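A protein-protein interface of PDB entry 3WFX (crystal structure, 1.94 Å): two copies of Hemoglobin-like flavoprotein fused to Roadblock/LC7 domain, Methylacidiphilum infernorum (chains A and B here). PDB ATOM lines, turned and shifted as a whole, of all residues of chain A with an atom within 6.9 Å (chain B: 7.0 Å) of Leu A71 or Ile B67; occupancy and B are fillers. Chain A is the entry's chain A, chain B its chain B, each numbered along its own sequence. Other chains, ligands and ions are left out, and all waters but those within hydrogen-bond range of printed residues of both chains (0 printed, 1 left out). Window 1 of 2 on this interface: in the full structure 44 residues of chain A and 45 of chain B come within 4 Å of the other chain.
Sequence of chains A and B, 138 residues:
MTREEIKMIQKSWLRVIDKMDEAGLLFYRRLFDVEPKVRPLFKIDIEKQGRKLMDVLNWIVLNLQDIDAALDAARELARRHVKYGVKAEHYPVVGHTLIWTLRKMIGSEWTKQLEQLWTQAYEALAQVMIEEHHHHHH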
ATOM      1  N   MET A   1     -27.253 -27.701  11.315  1.00  0.00           N
ATOM      2  CA  MET A   1     -28.188 -28.818  11.354  1.00  0.00           C
ATOM      3  C   MET A   1     -28.953 -28.977  10.064  1.00  0.00           C
ATOM      4  O   MET A   1     -29.148 -28.019   9.321  1.00  0.00           O
ATOM      5  CB  MET A   1     -29.207 -28.621  12.468  1.00  0.00           C
ATOM      6  CG  MET A   1     -28.674 -28.936  13.818  1.00  0.00           C
ATOM      7  SD  MET A   1     -29.962 -28.795  15.058  1.00  0.00           S
ATOM      8  CE  MET A   1     -28.952 -29.202  16.480  1.00  0.00           C
ATOM      9  N   ASP A  66     -34.296 -19.100  13.000  1.00  0.00           N
ATOM     10  CA  ASP A  66     -33.737 -17.846  12.468  1.00  0.00           C
ATOM     11  C   ASP A  66     -32.287 -17.992  12.034  1.00  0.00           C
ATOM     12  O   ASP A  66     -31.871 -17.441  10.998  1.00  0.00           O
ATOM     13  CB  ASP A  66     -33.802 -16.731  13.512  1.00  0.00           C
ATOM     14  CG  ASP A  66     -35.226 -16.273  13.796  1.00  0.00           C
ATOM     15  OD1 ASP A  66     -36.101 -16.501  12.936  1.00  0.00           O
ATOM     16  OD2 ASP A  66     -35.457 -15.674  14.870  1.00  0.00           O
ATOM     17  N   ILE A  67     -31.509 -18.698  12.848  1.00  0.00           N
ATOM     18  CA  ILE A  67     -30.096 -18.923  12.527  1.00  0.00           C
ATOM     19  C   ILE A  67     -29.977 -19.827  11.306  1.00  0.00           C
ATOM     20  O   ILE A  67     -29.109 -19.624  10.461  1.00  0.00           O
ATOM     21  CB  ILE A  67     -29.293 -19.533  13.710  1.00  0.00           C
ATOM     22  CG1 ILE A  67     -29.411 -18.654  14.955  1.00  0.00           C
ATOM     23  CG2 ILE A  67     -27.821 -19.663  13.333  1.00  0.00           C
ATOM     24  CD1 ILE A  67     -28.841 -17.262  14.777  1.00  0.00           C
ATOM     25  N   ASP A  68     -30.864 -20.813  11.200  1.00  0.00           N
ATOM     26  CA  ASP A  68     -30.838 -21.702  10.052  1.00  0.00           C
ATOM     27  C   ASP A  68     -31.087 -20.900   8.775  1.00  0.00           C
ATOM     28  O   ASP A  68     -30.359 -21.044   7.782  1.00  0.00           O
ATOM     29  CB  ASP A  68     -31.873 -22.818  10.177  1.00  0.00           C
ATOM     30  CG  ASP A  68     -31.715 -23.867   9.090  1.00  0.00           C
ATOM     31  OD1 ASP A  68     -30.619 -24.456   8.997  1.00  0.00           O
ATOM     32  OD2 ASP A  68     -32.677 -24.102   8.333  1.00  0.00           O
ATOM     33  N   ALA A  69     -32.110 -20.051   8.826  1.00  0.00           N
ATOM     34  CA  ALA A  69     -32.416 -19.116   7.745  1.00  0.00           C
ATOM     35  C   ALA A  69     -31.229 -18.242   7.376  1.00  0.00           C
ATOM     36  O   ALA A  69     -30.987 -17.988   6.195  1.00  0.00           O
ATOM     37  CB  ALA A  69     -33.598 -18.234   8.118  1.00  0.00           C
ATOM     38  N   ALA A  70     -30.499 -17.771   8.382  1.00  0.00           N
ATOM     39  CA  ALA A  70     -29.385 -16.863   8.142  1.00  0.00           C
ATOM     40  C   ALA A  70     -28.220 -17.583   7.447  1.00  0.00           C
ATOM     41  O   ALA A  70     -27.422 -16.974   6.739  1.00  0.00           O
ATOM     42  CB  ALA A  70     -28.929 -16.231   9.443  1.00  0.00           C
ATOM     43  N   LEU A  71     -28.140 -18.888   7.664  1.00  0.00           N
ATOM     44  CA  LEU A  71     -27.115 -19.725   7.054  1.00  0.00           C
ATOM     45  C   LEU A  71     -27.436 -20.051   5.594  1.00  0.00           C
ATOM     46  O   LEU A  71     -26.563 -20.491   4.851  1.00  0.00           O
ATOM     47  CB  LEU A  71     -26.972 -21.024   7.861  1.00  0.00           C
ATOM     48  CG  LEU A  71     -25.784 -21.232   8.810  1.00  0.00           C
ATOM     49  CD1 LEU A  71     -25.354 -19.954   9.506  1.00  0.00           C
ATOM     50  CD2 LEU A  71     -26.114 -22.313   9.835  1.00  0.00           C
ATOM     51  N   ASP A  72     -28.680 -19.831   5.167  1.00  0.00           N
ATOM     52  CA  ASP A  72     -29.077 -20.272   3.823  1.00  0.00           C
ATOM     53  C   ASP A  72     -28.362 -19.565   2.656  1.00  0.00           C
ATOM     54  O   ASP A  72     -28.206 -20.150   1.590  1.00  0.00           O
ATOM     55  CB  ASP A  72     -30.596 -20.232   3.640  1.00  0.00           C
ATOM     56  CG  ASP A  72     -31.300 -21.439   4.272  1.00  0.00           C
ATOM     57  OD1 ASP A  72     -30.649 -22.493   4.483  1.00  0.00           O
ATOM     58  OD2 ASP A  72     -32.512 -21.332   4.548  1.00  0.00           O
ATOM     59  N   ALA A  73     -27.939 -18.319   2.849  1.00  0.00           N
ATOM     60  CA  ALA A  73     -27.176 -17.612   1.811  1.00  0.00           C
ATOM     61  C   ALA A  73     -25.868 -18.333   1.510  1.00  0.00           C
ATOM     62  O   ALA A  73     -25.488 -18.501   0.350  1.00  0.00           O
ATOM     63  CB  ALA A  73     -26.903 -16.184   2.232  1.00  0.00           C
ATOM     64  N   ALA A  74     -25.170 -18.756   2.560  1.00  0.00           N
ATOM     65  CA  ALA A  74     -23.942 -19.523   2.372  1.00  0.00           C
ATOM     66  C   ALA A  74     -24.201 -20.881   1.715  1.00  0.00           C
ATOM     67  O   ALA A  74     -23.413 -21.334   0.884  1.00  0.00           O
ATOM     68  CB  ALA A  74     -23.201 -19.700   3.705  1.00  0.00           C
ATOM     69  N   ARG A  75     -25.291 -21.546   2.087  1.00  0.00           N
ATOM     70  CA  ARG A  75     -25.590 -22.825   1.451  1.00  0.00           C
ATOM     71  C   ARG A  75     -25.929 -22.609  -0.026  1.00  0.00           C
ATOM     72  O   ARG A  75     -25.578 -23.422  -0.865  1.00  0.00           O
ATOM     73  CB  ARG A  75     -26.754 -23.524   2.152  1.00  0.00           C
ATOM     74  CG  ARG A  75     -26.498 -23.824   3.621  1.00  0.00           C
ATOM     75  CD  ARG A  75     -27.735 -24.410   4.249  1.00  0.00           C
ATOM     76  NE  ARG A  75     -27.506 -24.760   5.641  1.00  0.00           N
ATOM     77  CZ  ARG A  75     -28.289 -24.361   6.635  1.00  0.00           C
ATOM     78  NH1 ARG A  75     -29.342 -23.594   6.378  1.00  0.00           N
ATOM     79  NH2 ARG A  75     -28.002 -24.718   7.875  1.00  0.00           N
ATOM     80  N   GLU A  76     -26.625 -21.510  -0.317  1.00  0.00           N
ATOM     81  CA  GLU A  76     -26.959 -21.117  -1.691  1.00  0.00           C
ATOM     82  C   GLU A  76     -25.674 -20.933  -2.492  1.00  0.00           C
ATOM     83  O   GLU A  76     -25.532 -21.437  -3.616  1.00  0.00           O
ATOM     84  CB  GLU A  76     -27.747 -19.798  -1.667  1.00  0.00           C
ATOM     85  CG  GLU A  76     -28.474 -19.440  -2.953  1.00  0.00           C
ATOM     86  CD  GLU A  76     -29.424 -18.244  -2.796  1.00  0.00           C
ATOM     87  OE1 GLU A  76     -30.410 -18.164  -3.556  1.00  0.00           O
ATOM     88  OE2 GLU A  76     -29.190 -17.379  -1.925  1.00  0.00           O
ATOM     89  N   VAL A 128     -19.564 -24.200   6.722  1.00  0.00           N
ATOM     90  CA  VAL A 128     -20.980 -24.260   6.348  1.00  0.00           C
ATOM     91  C   VAL A 128     -21.137 -24.650   4.876  1.00  0.00           C
ATOM     92  O   VAL A 128     -21.999 -25.457   4.521  1.00  0.00           O
ATOM     93  CB  VAL A 128     -21.695 -22.905   6.595  1.00  0.00           C
ATOM     94  CG1 VAL A 128     -23.057 -22.877   5.899  1.00  0.00           C
ATOM     95  CG2 VAL A 128     -21.849 -22.639   8.092  1.00  0.00           C
ATOM     96  N   GLU A 131     -20.183 -28.399   4.430  1.00  0.00           N
ATOM     97  CA  GLU A 131     -21.292 -29.239   4.865  1.00  0.00           C
ATOM     98  C   GLU A 131     -22.274 -29.396   3.707  1.00  0.00           C
ATOM     99  O   GLU A 131     -22.733 -30.495   3.406  1.00  0.00           O
ATOM    100  CB  GLU A 131     -21.990 -28.622   6.085  1.00  0.00           C
ATOM    101  CG  GLU A 131     -22.818 -29.612   6.892  1.00  0.00           C
ATOM    102  CD  GLU A 131     -23.556 -28.955   8.045  1.00  0.00           C
ATOM    103  OE1 GLU A 131     -23.344 -27.748   8.276  1.00  0.00           O
ATOM    104  OE2 GLU A 131     -24.353 -29.645   8.714  1.00  0.00           O
ATOM    105  N   TRP B  59     -18.682 -10.691  -0.626  1.00  0.00           N
ATOM    106  CA  TRP B  59     -19.613 -11.707  -0.157  1.00  0.00           C
ATOM    107  C   TRP B  59     -19.266 -12.063   1.277  1.00  0.00           C
ATOM    108  O   TRP B  59     -20.133 -12.064   2.160  1.00  0.00           O
ATOM    109  CB  TRP B  59     -19.578 -12.948  -1.055  1.00  0.00           C
ATOM    110  CG  TRP B  59     -20.841 -13.754  -0.985  1.00  0.00           C
ATOM    111  CD1 TRP B  59     -21.853 -13.786  -1.906  1.00  0.00           C
ATOM    112  CD2 TRP B  59     -21.242 -14.623   0.081  1.00  0.00           C
ATOM    113  NE1 TRP B  59     -22.857 -14.628  -1.475  1.00  0.00           N
ATOM    114  CE2 TRP B  59     -22.506 -15.149  -0.257  1.00  0.00           C
ATOM    115  CE3 TRP B  59     -20.648 -15.016   1.283  1.00  0.00           C
ATOM    116  CZ2 TRP B  59     -23.176 -16.053   0.558  1.00  0.00           C
ATOM    117  CZ3 TRP B  59     -21.328 -15.912   2.100  1.00  0.00           C
ATOM    118  CH2 TRP B  59     -22.572 -16.417   1.732  1.00  0.00           C
ATOM    119  N   LEU B  62     -20.048  -8.978   3.774  1.00  0.00           N
ATOM    120  CA  LEU B  62     -21.470  -8.658   3.941  1.00  0.00           C
ATOM    121  C   LEU B  62     -22.195  -9.787   4.661  1.00  0.00           C
ATOM    122  O   LEU B  62     -23.046  -9.553   5.519  1.00  0.00           O
ATOM    123  CB  LEU B  62     -22.146  -8.392   2.597  1.00  0.00           C
ATOM    124  CG  LEU B  62     -21.586  -7.181   1.834  1.00  0.00           C
ATOM    125  CD1 LEU B  62     -22.429  -6.850   0.615  1.00  0.00           C
ATOM    126  CD2 LEU B  62     -21.440  -5.975   2.741  1.00  0.00           C
ATOM    127  N   ASN B  63     -21.864 -11.016   4.289  1.00  0.00           N
ATOM    128  CA  ASN B  63     -22.423 -12.174   4.962  1.00  0.00           C
ATOM    129  C   ASN B  63     -22.004 -12.191   6.422  1.00  0.00           C
ATOM    130  O   ASN B  63     -22.804 -12.523   7.306  1.00  0.00           O
ATOM    131  CB  ASN B  63     -21.995 -13.461   4.270  1.00  0.00           C
ATOM    132  CG  ASN B  63     -22.576 -14.678   4.938  1.00  0.00           C
ATOM    133  OD1 ASN B  63     -23.777 -14.956   4.813  1.00  0.00           O
ATOM    134  ND2 ASN B  63     -21.739 -15.408   5.662  1.00  0.00           N
ATOM    135  N   LEU B  64     -20.757 -11.802   6.680  1.00  0.00           N
ATOM    136  CA  LEU B  64     -20.278 -11.682   8.061  1.00  0.00           C
ATOM    137  C   LEU B  64     -21.115 -10.684   8.848  1.00  0.00           C
ATOM    138  O   LEU B  64     -21.460 -10.917  10.009  1.00  0.00           O
ATOM    139  CB  LEU B  64     -18.797 -11.280   8.089  1.00  0.00           C
ATOM    140  CG  LEU B  64     -18.207 -10.804   9.414  1.00  0.00           C
ATOM    141  CD1 LEU B  64     -18.246 -11.923  10.461  1.00  0.00           C
ATOM    142  CD2 LEU B  64     -16.775 -10.301   9.225  1.00  0.00           C
ATOM    143  N   GLN B  65     -21.453  -9.566   8.213  1.00  0.00           N
ATOM    144  CA  GLN B  65     -22.326  -8.587   8.847  1.00  0.00           C
ATOM    145  C   GLN B  65     -23.728  -9.163   9.076  1.00  0.00           C
ATOM    146  O   GLN B  65     -24.365  -8.894  10.110  1.00  0.00           O
ATOM    147  CB  GLN B  65     -22.387  -7.302   8.001  1.00  0.00           C
ATOM    148  CG  GLN B  65     -21.035  -6.613   7.872  1.00  0.00           C
ATOM    149  CD  GLN B  65     -21.026  -5.489   6.841  1.00  0.00           C
ATOM    150  OE1 GLN B  65     -21.895  -5.413   5.970  1.00  0.00           O
ATOM    151  NE2 GLN B  65     -20.040  -4.610   6.945  1.00  0.00           N
ATOM    152  N   ASP B  66     -24.216  -9.945   8.117  1.00  0.00           N
ATOM    153  CA  ASP B  66     -25.554 -10.531   8.238  1.00  0.00           C
ATOM    154  C   ASP B  66     -25.625 -11.535   9.403  1.00  0.00           C
ATOM    155  O   ASP B  66     -26.595 -11.558  10.182  1.00  0.00           O
ATOM    156  CB  ASP B  66     -25.988 -11.226   6.940  1.00  0.00           C
ATOM    157  CG  ASP B  66     -26.384 -10.249   5.834  1.00  0.00           C
ATOM    158  OD1 ASP B  66     -26.580  -9.042   6.094  1.00  0.00           O
ATOM    159  OD2 ASP B  66     -26.517 -10.708   4.682  1.00  0.00           O
ATOM    160  N   ILE B  67     -24.599 -12.368   9.522  1.00  0.00           N
ATOM    161  CA  ILE B  67     -24.549 -13.366  10.595  1.00  0.00           C
ATOM    162  C   ILE B  67     -24.426 -12.695  11.961  1.00  0.00           C
ATOM    163  O   ILE B  67     -25.113 -13.063  12.923  1.00  0.00           O
ATOM    164  CB  ILE B  67     -23.388 -14.373  10.388  1.00  0.00           C
ATOM    165  CG1 ILE B  67     -23.571 -15.115   9.075  1.00  0.00           C
ATOM    166  CG2 ILE B  67     -23.364 -15.389  11.518  1.00  0.00           C
ATOM    167  CD1 ILE B  67     -24.733 -16.095   9.090  1.00  0.00           C
ATOM    168  N   ASP B  68     -23.555 -11.698  12.041  1.00  0.00           N
ATOM    169  CA  ASP B  68     -23.430 -10.932  13.264  1.00  0.00           C
ATOM    170  C   ASP B  68     -24.775 -10.338  13.699  1.00  0.00           C
ATOM    171  O   ASP B  68     -25.088 -10.340  14.885  1.00  0.00           O
ATOM    172  CB  ASP B  68     -22.399  -9.818  13.128  1.00  0.00           C
ATOM    173  CG  ASP B  68     -22.170  -9.095  14.441  1.00  0.00           C
ATOM    174  OD1 ASP B  68     -21.560  -9.707  15.339  1.00  0.00           O
ATOM    175  OD2 ASP B  68     -22.608  -7.934  14.578  1.00  0.00           O
ATOM    176  N   ALA B  69     -25.566  -9.842  12.748  1.00  0.00           N
ATOM    177  CA  ALA B  69     -26.909  -9.326  13.064  1.00  0.00           C
ATOM    178  C   ALA B  69     -27.845 -10.419  13.555  1.00  0.00           C
ATOM    179  O   ALA B  69     -28.724 -10.184  14.408  1.00  0.00           O
ATOM    180  CB  ALA B  69     -27.526  -8.631  11.851  1.00  0.00           C
ATOM    181  N   ALA B  70     -27.678 -11.613  13.005  1.00  0.00           N
ATOM    182  CA  ALA B  70     -28.514 -12.740  13.398  1.00  0.00           C
ATOM    183  C   ALA B  70     -28.221 -13.183  14.837  1.00  0.00           C
ATOM    184  O   ALA B  70     -29.099 -13.713  15.516  1.00  0.00           O
ATOM    185  CB  ALA B  70     -28.347 -13.897  12.424  1.00  0.00           C
ATOM    186  N   LEU B  71     -27.000 -12.946  15.300  1.00  0.00           N
ATOM    187  CA  LEU B  71     -26.612 -13.283  16.677  1.00  0.00           C
ATOM    188  C   LEU B  71     -27.063 -12.253  17.733  1.00  0.00           C
ATOM    189  O   LEU B  71     -26.998 -12.520  18.940  1.00  0.00           O
ATOM    190  CB  LEU B  71     -25.094 -13.497  16.772  1.00  0.00           C
ATOM    191  CG  LEU B  71     -24.511 -14.680  15.990  1.00  0.00           C
ATOM    192  CD1 LEU B  71     -22.999 -14.793  16.189  1.00  0.00           C
ATOM    193  CD2 LEU B  71     -25.203 -15.976  16.353  1.00  0.00           C
ATOM    194  N   ASP B  72     -27.524 -11.085  17.291  1.00  0.00           N
ATOM    195  CA  ASP B  72     -27.891 -10.022  18.229  1.00  0.00           C
ATOM    196  C   ASP B  72     -29.046 -10.391  19.170  1.00  0.00           C
ATOM    197  O   ASP B  72     -29.030  -9.994  20.326  1.00  0.00           O
ATOM    198  CB  ASP B  72     -28.171  -8.689  17.513  1.00  0.00           C
ATOM    199  CG  ASP B  72     -26.888  -7.942  17.145  1.00  0.00           C
ATOM    200  OD1 ASP B  72     -25.834  -8.212  17.763  1.00  0.00           O
ATOM    201  OD2 ASP B  72     -26.939  -7.078  16.245  1.00  0.00           O
ATOM    202  N   ARG B  75     -27.544 -12.249  21.989  1.00  0.00           N
ATOM    203  CA  ARG B  75     -26.794 -11.297  22.793  1.00  0.00           C
ATOM    204  C   ARG B  75     -27.714 -10.396  23.632  1.00  0.00           C
ATOM    205  O   ARG B  75     -27.395 -10.122  24.780  1.00  0.00           O
ATOM    206  CB  ARG B  75     -25.861 -10.464  21.917  1.00  0.00           C
ATOM    207  CG  ARG B  75     -24.814 -11.298  21.193  1.00  0.00           C
ATOM    208  CD  ARG B  75     -23.835 -10.398  20.412  1.00  0.00           C
ATOM    209  NE  ARG B  75     -22.773 -11.168  19.790  1.00  0.00           N
ATOM    210  CZ  ARG B  75     -22.540 -11.199  18.480  1.00  0.00           C
ATOM    211  NH1 ARG B  75     -23.306 -10.506  17.645  1.00  0.00           N
ATOM    212  NH2 ARG B  75     -21.548 -11.934  18.006  1.00  0.00           N
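Among the printed residues, merely in contact across the chains: Ile A67 with Ala B70 (3.6 Å), Ala A70 with Ile B67 (3.7 Å), Ala A70 with Ala B70 (3.8 Å), Leu A71 with Ile B67 (3.9 Å), Ala A73 with Trp B59 (3.4 Å) and Ala A74 with Trp B59 (3.5 Å).
Of the printed residues of chain B, Ile A67 touches Ala B70 (3.6 Å). Printed residues of chain B within 4 Å of Ala A70: Ile B67 and Ala B70. Of chain B, only Ile B67 comes within 4 Å of Leu A71. Ile B67 touches two residues of chain A. The nearest residue of chain B that does not touch Leu A71 is Asn B63 (6.2 Å). The nearest residue of chain A that does not touch Ile B67 is Ile A67 (5.8 Å). The nearest printed residue of chain A that does not touch Trp B59 is Arg A75 (5.8 Å).
Hydrophobic or aromatic side chains of chain A within 4 Å of the printed part of chain B: Ile A67, Ala A70, Leu A71 and Ala A74. Along chain A the printed residues that touch a printed residue of chain B span positions 67 to 74. Printed residues of chain B that touch a printed residue of chain A: Trp B59, Ile B67 and Ala B70. Hydrophobic or aromatic side chains of chain B that line the printed part of chain A: Trp B59, Ile B67 and Ala B70.
Ile A67 touches Ala B70, and with the chains exchanged Ala A70 touches Ile B67. Ala B70 touches its own counterpart, Ala A70. Leu A71 touches Ile B67, but with the chains exchanged Ile A67 does not touch Leu B71 (4.2 Å). 8 positions are printed for both chains. Of the 6 pairs that touch across the chains among the printed residues, 3 have their exchanged pair printed and touching as well.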
